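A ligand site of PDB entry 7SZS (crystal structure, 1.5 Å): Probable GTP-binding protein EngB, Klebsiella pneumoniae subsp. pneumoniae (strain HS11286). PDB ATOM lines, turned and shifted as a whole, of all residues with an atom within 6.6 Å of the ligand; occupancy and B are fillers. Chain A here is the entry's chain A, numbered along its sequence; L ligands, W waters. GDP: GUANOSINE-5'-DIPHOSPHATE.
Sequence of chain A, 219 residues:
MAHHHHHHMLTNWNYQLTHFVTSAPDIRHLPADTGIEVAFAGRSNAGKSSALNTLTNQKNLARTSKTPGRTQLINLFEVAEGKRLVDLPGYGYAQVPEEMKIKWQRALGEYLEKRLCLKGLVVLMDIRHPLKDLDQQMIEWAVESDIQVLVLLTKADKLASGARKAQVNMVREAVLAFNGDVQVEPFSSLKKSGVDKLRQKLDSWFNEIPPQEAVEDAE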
ATOM      1  N   GLY A  42     -21.522   4.161  10.849  1.00  0.00           N
ATOM      2  CA  GLY A  42     -20.550   3.921  11.916  1.00  0.00           C
ATOM      3  C   GLY A  42     -19.238   4.608  11.617  1.00  0.00           C
ATOM      4  O   GLY A  42     -19.029   5.153  10.533  1.00  0.00           O
ATOM      5  N   ARG A  43     -18.357   4.581  12.607  1.00  0.00           N
ATOM      6  CA  ARG A  43     -17.001   5.090  12.379  1.00  0.00           C
ATOM      7  C   ARG A  43     -16.326   4.265  11.300  1.00  0.00           C
ATOM      8  O   ARG A  43     -16.531   3.043  11.224  1.00  0.00           O
ATOM      9  CB  ARG A  43     -16.189   5.013  13.675  1.00  0.00           C
ATOM     10  CG  ARG A  43     -16.610   6.014  14.746  1.00  0.00           C
ATOM     11  CD  ARG A  43     -16.036   5.646  16.124  1.00  0.00           C
ATOM     12  NE  ARG A  43     -14.589   5.791  16.159  1.00  0.00           N
ATOM     13  CZ  ARG A  43     -13.836   5.267  17.113  1.00  0.00           C
ATOM     14  NH1 ARG A  43     -14.362   4.538  18.078  1.00  0.00           N
ATOM     15  NH2 ARG A  43     -12.519   5.457  17.072  1.00  0.00           N
ATOM     16  N   SER A  44     -15.541   4.921  10.444  1.00  0.00           N
ATOM     17  CA  SER A  44     -14.694   4.178   9.518  1.00  0.00           C
ATOM     18  C   SER A  44     -13.909   3.125  10.286  1.00  0.00           C
ATOM     19  O   SER A  44     -13.393   3.388  11.378  1.00  0.00           O
ATOM     20  CB  SER A  44     -13.751   5.125   8.787  1.00  0.00           C
ATOM     21  OG  SER A  44     -14.479   6.094   8.043  1.00  0.00           O
ATOM     22  N   ASN A  45     -13.849   1.914   9.732  1.00  0.00           N
ATOM     23  CA  ASN A  45     -13.171   0.735  10.267  1.00  0.00           C
ATOM     24  C   ASN A  45     -13.961   0.025  11.365  1.00  0.00           C
ATOM     25  O   ASN A  45     -13.449  -0.942  11.932  1.00  0.00           O
ATOM     26  CB  ASN A  45     -11.765   1.041  10.812  1.00  0.00           C
ATOM     27  CG  ASN A  45     -10.777  -0.060  10.514  1.00  0.00           C
ATOM     28  OD1 ASN A  45     -10.661  -0.504   9.361  1.00  0.00           O
ATOM     29  ND2 ASN A  45     -10.060  -0.502  11.528  1.00  0.00           N
ATOM     30  N   ALA A  46     -15.186   0.444  11.678  1.00  0.00           N
ATOM     31  CA  ALA A  46     -15.935  -0.244  12.726  1.00  0.00           C
ATOM     32  C   ALA A  46     -16.413  -1.623  12.273  1.00  0.00           C
ATOM     33  O   ALA A  46     -16.768  -2.453  13.123  1.00  0.00           O
ATOM     34  CB  ALA A  46     -17.140   0.582  13.174  1.00  0.00           C
ATOM     35  N   GLY A  47     -16.448  -1.886  10.974  1.00  0.00           N
ATOM     36  CA  GLY A  47     -16.912  -3.161  10.473  1.00  0.00           C
ATOM     37  C   GLY A  47     -18.208  -3.111   9.688  1.00  0.00           C
ATOM     38  O   GLY A  47     -18.893  -4.145   9.600  1.00  0.00           O
ATOM     39  N   LYS A  48     -18.555  -1.956   9.128  1.00  0.00           N
ATOM     40  CA  LYS A  48     -19.830  -1.796   8.443  1.00  0.00           C
ATOM     41  C   LYS A  48     -19.893  -2.574   7.129  1.00  0.00           C
ATOM     42  O   LYS A  48     -20.874  -3.285   6.867  1.00  0.00           O
ATOM     43  CB  LYS A  48     -20.118  -0.308   8.207  1.00  0.00           C
ATOM     44  CG  LYS A  48     -21.364  -0.025   7.379  1.00  0.00           C
ATOM     45  CD  LYS A  48     -21.922   1.392   7.628  1.00  0.00           C
ATOM     46  CE  LYS A  48     -20.920   2.506   7.347  1.00  0.00           C
ATOM     47  NZ  LYS A  48     -20.403   2.480   5.945  1.00  0.00           N
ATOM     48  N   SER A  49     -18.853  -2.468   6.288  1.00  0.00           N
ATOM     49  CA  SER A  49     -18.906  -3.200   5.025  1.00  0.00           C
ATOM     50  C   SER A  49     -18.897  -4.700   5.270  1.00  0.00           C
ATOM     51  O   SER A  49     -19.620  -5.444   4.584  1.00  0.00           O
ATOM     52  CB  SER A  49     -17.747  -2.791   4.106  1.00  0.00           C
ATOM     53  OG  SER A  49     -16.493  -3.104   4.672  1.00  0.00           O
ATOM     54  N   SER A  50     -18.108  -5.165   6.243  1.00  0.00           N
ATOM     55  CA  SER A  50     -18.084  -6.589   6.549  1.00  0.00           C
ATOM     56  C   SER A  50     -19.446  -7.081   7.005  1.00  0.00           C
ATOM     57  O   SER A  50     -19.878  -8.181   6.640  1.00  0.00           O
ATOM     58  CB  SER A  50     -17.031  -6.877   7.613  1.00  0.00           C
ATOM     59  OG  SER A  50     -15.730  -6.583   7.133  1.00  0.00           O
ATOM     60  N   ALA A  51     -20.156  -6.275   7.797  1.00  0.00           N
ATOM     61  CA  ALA A  51     -21.470  -6.678   8.274  1.00  0.00           C
ATOM     62  C   ALA A  51     -22.460  -6.790   7.131  1.00  0.00           C
ATOM     63  O   ALA A  51     -23.241  -7.741   7.066  1.00  0.00           O
ATOM     64  CB  ALA A  51     -21.972  -5.683   9.318  1.00  0.00           C
ATOM     65  N   ASN A  53     -21.671  -7.265   3.946  1.00  0.00           N
ATOM     66  CA  ASN A  53     -21.240  -8.416   3.161  1.00  0.00           C
ATOM     67  C   ASN A  53     -21.708  -9.714   3.799  1.00  0.00           C
ATOM     68  O   ASN A  53     -22.118 -10.643   3.093  1.00  0.00           O
ATOM     69  CB  ASN A  53     -19.717  -8.420   3.025  1.00  0.00           C
ATOM     70  CG  ASN A  53     -19.178  -7.283   2.189  1.00  0.00           C
ATOM     71  OD1 ASN A  53     -19.922  -6.647   1.430  1.00  0.00           O
ATOM     72  ND2 ASN A  53     -17.875  -7.024   2.306  1.00  0.00           N
ATOM     73  N   GLY A  90     -18.770   6.204   6.240  1.00  0.00           N
ATOM     74  CA  GLY A  90     -18.270   6.156   7.601  1.00  0.00           C
ATOM     75  C   GLY A  90     -17.744   7.501   8.074  1.00  0.00           C
ATOM     76  O   GLY A  90     -17.181   8.279   7.300  1.00  0.00           O
ATOM     77  N   LEU A 124     -23.149   0.792  13.826  1.00  0.00           N
ATOM     78  CA  LEU A 124     -22.134  -0.227  14.110  1.00  0.00           C
ATOM     79  C   LEU A 124     -20.993   0.432  14.854  1.00  0.00           C
ATOM     80  O   LEU A 124     -20.500   1.501  14.451  1.00  0.00           O
ATOM     81  CB  LEU A 124     -21.638  -0.875  12.824  1.00  0.00           C
ATOM     82  CG  LEU A 124     -22.765  -1.570  12.033  1.00  0.00           C
ATOM     83  CD1 LEU A 124     -23.300  -0.698  10.864  1.00  0.00           C
ATOM     84  CD2 LEU A 124     -22.344  -2.947  11.572  1.00  0.00           C
ATOM     85  N   THR A 154     -19.742  -4.486  17.182  1.00  0.00           N
ATOM     86  CA  THR A 154     -19.034  -5.292  16.205  1.00  0.00           C
ATOM     87  C   THR A 154     -17.734  -5.842  16.776  1.00  0.00           C
ATOM     88  O   THR A 154     -17.248  -5.418  17.826  1.00  0.00           O
ATOM     89  CB  THR A 154     -18.734  -4.482  14.948  1.00  0.00           C
ATOM     90  OG1 THR A 154     -18.013  -3.297  15.324  1.00  0.00           O
ATOM     91  CG2 THR A 154     -20.029  -4.081  14.227  1.00  0.00           C
ATOM     92  N   LYS A 155     -17.158  -6.792  16.020  1.00  0.00           N
ATOM     93  CA  LYS A 155     -15.901  -7.440  16.392  1.00  0.00           C
ATOM     94  C   LYS A 155     -16.042  -8.123  17.755  1.00  0.00           C
ATOM     95  O   LYS A 155     -15.067  -8.214  18.520  1.00  0.00           O
ATOM     96  CB  LYS A 155     -14.737  -6.445  16.370  1.00  0.00           C
ATOM     97  CG  LYS A 155     -14.700  -5.636  15.054  1.00  0.00           C
ATOM     98  CD  LYS A 155     -13.482  -4.718  14.935  1.00  0.00           C
ATOM     99  CE  LYS A 155     -13.590  -3.856  13.686  1.00  0.00           C
ATOM    100  NZ  LYS A 155     -12.409  -2.936  13.549  1.00  0.00           N
ATOM    101  N   ALA A 156     -17.243  -8.631  18.031  1.00  0.00           N
ATOM    102  CA  ALA A 156     -17.543  -9.213  19.336  1.00  0.00           C
ATOM    103  C   ALA A 156     -16.728 -10.478  19.595  1.00  0.00           C
ATOM    104  O   ALA A 156     -16.577 -10.868  20.762  1.00  0.00           O
ATOM    105  CB  ALA A 156     -19.043  -9.517  19.458  1.00  0.00           C
ATOM    106  N   ASP A 157     -16.178 -11.095  18.543  1.00  0.00           N
ATOM    107  CA  ASP A 157     -15.276 -12.240  18.680  1.00  0.00           C
ATOM    108  C   ASP A 157     -13.954 -11.890  19.358  1.00  0.00           C
ATOM    109  O   ASP A 157     -13.219 -12.810  19.733  1.00  0.00           O
ATOM    110  CB  ASP A 157     -14.987 -12.807  17.301  1.00  0.00           C
ATOM    111  CG  ASP A 157     -14.433 -11.765  16.351  1.00  0.00           C
ATOM    112  OD1 ASP A 157     -15.237 -11.034  15.760  1.00  0.00           O
ATOM    113  OD2 ASP A 157     -13.192 -11.645  16.260  1.00  0.00           O
ATOM    114  N   LYS A 158     -13.630 -10.613  19.494  1.00  0.00           N
ATOM    115  CA  LYS A 158     -12.397 -10.215  20.155  1.00  0.00           C
ATOM    116  C   LYS A 158     -12.479 -10.290  21.672  1.00  0.00           C
ATOM    117  O   LYS A 158     -11.451 -10.144  22.343  1.00  0.00           O
ATOM    118  CB  LYS A 158     -12.011  -8.795  19.727  1.00  0.00           C
ATOM    119  CG  LYS A 158     -11.580  -8.717  18.274  1.00  0.00           C
ATOM    120  CD  LYS A 158     -11.092  -7.340  17.912  1.00  0.00           C
ATOM    121  CE  LYS A 158     -10.466  -7.294  16.520  1.00  0.00           C
ATOM    122  NZ  LYS A 158      -9.082  -7.869  16.485  1.00  0.00           N
ATOM    123  N   PHE A 187     -22.166  -8.514  17.722  1.00  0.00           N
ATOM    124  CA  PHE A 187     -22.146  -8.915  16.325  1.00  0.00           C
ATOM    125  C   PHE A 187     -20.715  -9.282  15.935  1.00  0.00           C
ATOM    126  O   PHE A 187     -19.755  -8.631  16.362  1.00  0.00           O
ATOM    127  CB  PHE A 187     -22.676  -7.770  15.434  1.00  0.00           C
ATOM    128  CG  PHE A 187     -22.917  -8.179  14.008  1.00  0.00           C
ATOM    129  CD1 PHE A 187     -21.903  -8.102  13.059  1.00  0.00           C
ATOM    130  CD2 PHE A 187     -24.185  -8.585  13.595  1.00  0.00           C
ATOM    131  CE1 PHE A 187     -22.137  -8.478  11.749  1.00  0.00           C
ATOM    132  CE2 PHE A 187     -24.410  -8.943  12.276  1.00  0.00           C
ATOM    133  CZ  PHE A 187     -23.390  -8.885  11.349  1.00  0.00           C
ATOM    134  N   SER A 188     -20.584 -10.345  15.137  1.00  0.00           N
ATOM    135  CA  SER A 188     -19.282 -10.690  14.558  1.00  0.00           C
ATOM    136  C   SER A 188     -19.457 -11.137  13.114  1.00  0.00           C
ATOM    137  O   SER A 188     -19.999 -12.215  12.851  1.00  0.00           O
ATOM    138  CB  SER A 188     -18.585 -11.791  15.355  1.00  0.00           C
ATOM    139  OG  SER A 188     -17.396 -12.193  14.708  1.00  0.00           O
ATOM    140  N   SER A 189     -18.977 -10.319  12.174  1.00  0.00           N
ATOM    141  CA  SER A 189     -18.868 -10.768  10.793  1.00  0.00           C
ATOM    142  C   SER A 189     -17.953 -11.973  10.678  1.00  0.00           C
ATOM    143  O   SER A 189     -18.211 -12.894   9.898  1.00  0.00           O
ATOM    144  CB  SER A 189     -18.356  -9.635   9.896  1.00  0.00           C
ATOM    145  OG  SER A 189     -19.305  -8.596   9.846  1.00  0.00           O
ATOM    146  N   LEU A 190     -16.861 -11.985  11.445  1.00  0.00           N
ATOM    147  CA  LEU A 190     -15.868 -13.039  11.299  1.00  0.00           C
ATOM    148  C   LEU A 190     -16.439 -14.397  11.668  1.00  0.00           C
ATOM    149  O   LEU A 190     -16.220 -15.379  10.952  1.00  0.00           O
ATOM    150  CB  LEU A 190     -14.645 -12.709  12.160  1.00  0.00           C
ATOM    151  CG  LEU A 190     -13.532 -13.753  12.216  1.00  0.00           C
ATOM    152  CD1 LEU A 190     -12.884 -13.910  10.842  1.00  0.00           C
ATOM    153  CD2 LEU A 190     -12.506 -13.352  13.269  1.00  0.00           C
ATOM    154  N   LYS A 191     -17.196 -14.473  12.762  1.00  0.00           N
ATOM    155  CA  LYS A 191     -17.774 -15.718  13.234  1.00  0.00           C
ATOM    156  C   LYS A 191     -19.226 -15.887  12.795  1.00  0.00           C
ATOM    157  O   LYS A 191     -19.867 -16.862  13.189  1.00  0.00           O
ATOM    158  CB  LYS A 191     -17.683 -15.789  14.761  1.00  0.00           C
ATOM    159  CG  LYS A 191     -16.266 -15.687  15.290  1.00  0.00           C
ATOM    160  CD  LYS A 191     -15.397 -16.806  14.728  1.00  0.00           C
ATOM    161  CE  LYS A 191     -14.019 -16.830  15.366  1.00  0.00           C
ATOM    162  NZ  LYS A 191     -13.224 -18.001  14.910  1.00  0.00           N
HETATM  163  PB  GDP L   1     -15.687  -0.428   7.603  1.00  0.00           P
HETATM  164  O1B GDP L   1     -16.477  -0.818   6.403  1.00  0.00           O
HETATM  165  O2B GDP L   1     -16.574   0.012   8.765  1.00  0.00           O
HETATM  166  O3B GDP L   1     -14.644   0.671   7.318  1.00  0.00           O
HETATM  167  O3A GDP L   1     -14.903  -1.698   8.151  1.00  0.00           O
HETATM  168  PA  GDP L   1     -14.567  -3.117   7.510  1.00  0.00           P
HETATM  169  O1A GDP L   1     -15.770  -3.989   7.424  1.00  0.00           O
HETATM  170  O2A GDP L   1     -13.790  -2.883   6.220  1.00  0.00           O
HETATM  171  O5' GDP L   1     -13.606  -3.738   8.589  1.00  0.00           O
HETATM  172  C5' GDP L   1     -12.441  -3.012   9.051  1.00  0.00           C
HETATM  173  C4' GDP L   1     -11.457  -3.984   9.641  1.00  0.00           C
HETATM  174  O4' GDP L   1     -12.065  -4.679  10.754  1.00  0.00           O
HETATM  175  C3' GDP L   1     -10.942  -5.071   8.691  1.00  0.00           C
HETATM  176  O3' GDP L   1      -9.585  -5.393   8.990  1.00  0.00           O
HETATM  177  C2' GDP L   1     -11.840  -6.250   9.018  1.00  0.00           C
HETATM  178  O2' GDP L   1     -11.262  -7.504   8.714  1.00  0.00           O
HETATM  179  C1' GDP L   1     -12.017  -6.074  10.526  1.00  0.00           C
HETATM  180  N9  GDP L   1     -13.270  -6.645  11.007  1.00  0.00           N
HETATM  181  C8  GDP L   1     -14.521  -6.364  10.516  1.00  0.00           C
HETATM  182  N7  GDP L   1     -15.460  -7.077  11.086  1.00  0.00           N
HETATM  183  C5  GDP L   1     -14.792  -7.880  11.998  1.00  0.00           C
HETATM  184  C6  GDP L   1     -15.271  -8.854  12.905  1.00  0.00           C
HETATM  185  O6  GDP L   1     -16.435  -9.229  13.042  1.00  0.00           O
HETATM  186  N1  GDP L   1     -14.260  -9.403  13.670  1.00  0.00           N
HETATM  187  C2  GDP L   1     -12.938  -9.059  13.577  1.00  0.00           C
HETATM  188  N2  GDP L   1     -12.103  -9.662  14.430  1.00  0.00           N
HETATM  189  N3  GDP L   1     -12.470  -8.160  12.715  1.00  0.00           N
HETATM  190  C4  GDP L   1     -13.444  -7.612  11.967  1.00  0.00           C
HETATM  191  O   HOH W   1     -17.797   2.341   8.712  1.00  0.00           O
HETATM  192  O   HOH W   2      -9.864  -7.157  13.221  1.00  0.00           O
HETATM  193  O   HOH W   3     -18.234   0.832   5.152  1.00  0.00           O
HETATM  194  O   HOH W   4     -18.334  -7.495  13.399  1.00  0.00           O
HETATM  195  O   HOH W   5     -14.360   2.500   5.760  1.00  0.00           O
HETATM  196  O   HOH W   6      -9.307  -9.816  14.256  1.00  0.00           O
HETATM  197  O   HOH W   7     -18.234  -6.412  10.970  1.00  0.00           O
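The backbone NH (N) of Ser 50 lies within hydrogen-bond range of an oxygen (O1A) of the ligand (2.9 Å). The side-chain hydroxyl (OG) of Ser 50 sits at hydrogen-bond distance from an oxygen (O1A) of the ligand, 2.6 Å away. N of Lys 48 sits at hydrogen-bond distance from O2B of the ligand (2.8 Å). The side-chain carboxylate (OD1) of Asp 157 sits at hydrogen-bond distance from a nitrogen (N1) of the ligand. O3B of the ligand lies within hydrogen-bond range of N of Asn 45, 2.8 Å away. The backbone NH (N) of Ser 49 lies within hydrogen-bond range of an oxygen (O1B) of the ligand, 2.9 Å away. The side-chain hydroxyl of Ser 49 sits at hydrogen-bond distance from an oxygen (O1B) of the ligand, at 2.9 Å. N of Ser 189 sits at hydrogen-bond distance from O6 of the ligand, 2.9 Å away. The backbone NH of Gly 47 sits at hydrogen-bond distance from an oxygen (O2B) of the ligand. N of Leu 190 sits at hydrogen-bond distance from O6 of the ligand (3.2 Å). The backbone NH (N) of Ala 46 is in hydrogen-bond range of an oxygen (O2B) of the ligand (3.3 Å). NZ of Lys 155 is in hydrogen-bond range of O4' of the ligand (3.3 Å).
Water W4 lies within hydrogen-bond range of O6 of the ligand (2.6 Å), N of Lys 155 (3.0 Å), N of Ser 189 (3.1 Å) and O of Phe 187 (3.5 Å). Water W1 lies within hydrogen-bond range of an oxygen (O2B) of the ligand and the backbone carbonyl oxygen (O) of Arg 43. Water W3 bridges O1B of the ligand (2.7 Å) and NZ of Lys 48 (2.8 Å). Water W6 bridges a nitrogen (N2) of the ligand and the side-chain amino group of Lys 158. Water W2 lies within hydrogen-bond range of N3 of the ligand (2.8 Å) and NZ of Lys 158 (3.4 Å). Water W7 lies within hydrogen-bond range of the side-chain hydroxyl (OG) of Ser 189, the backbone carbonyl oxygen (O) of Gly 47 and a nitrogen (N7) of the ligand.
Arg 43 touches the ligand (O to O2B, 3.9 Å). Ser 44 touches the ligand (C to O3B, 3.9 Å). CE of Lys 158 touches N2 of the ligand, 3.6 Å away. OG of Ser 188 touches O6 of the ligand, 3.5 Å away.
The backbone carbonyl oxygen of Ser 50 sits close to the side-chain hydroxyl of Ser 189 (3.3 Å). OD1 of Asp 157 lies within hydrogen-bond range of OG of Ser 188. The backbone carbonyl oxygen (O) of Ser 49 lies close to the side-chain amide nitrogen (ND2) of Asn 53, 3.3 Å away. The side-chain hydroxyl (OG) of Ser 189 is in hydrogen-bond range of the backbone NH (N) of Ala 51 (3.2 Å). N of Leu 190 lies close to OG of Ser 188. The backbone carbonyl oxygen (O) of Ala 46 sits at hydrogen-bond distance from the side-chain hydroxyl (OG1) of Thr 154, at 2.7 Å. N of Lys 155 is in hydrogen-bond range of O of Phe 187. N of Lys 191 is in hydrogen-bond range of OG of Ser 188.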
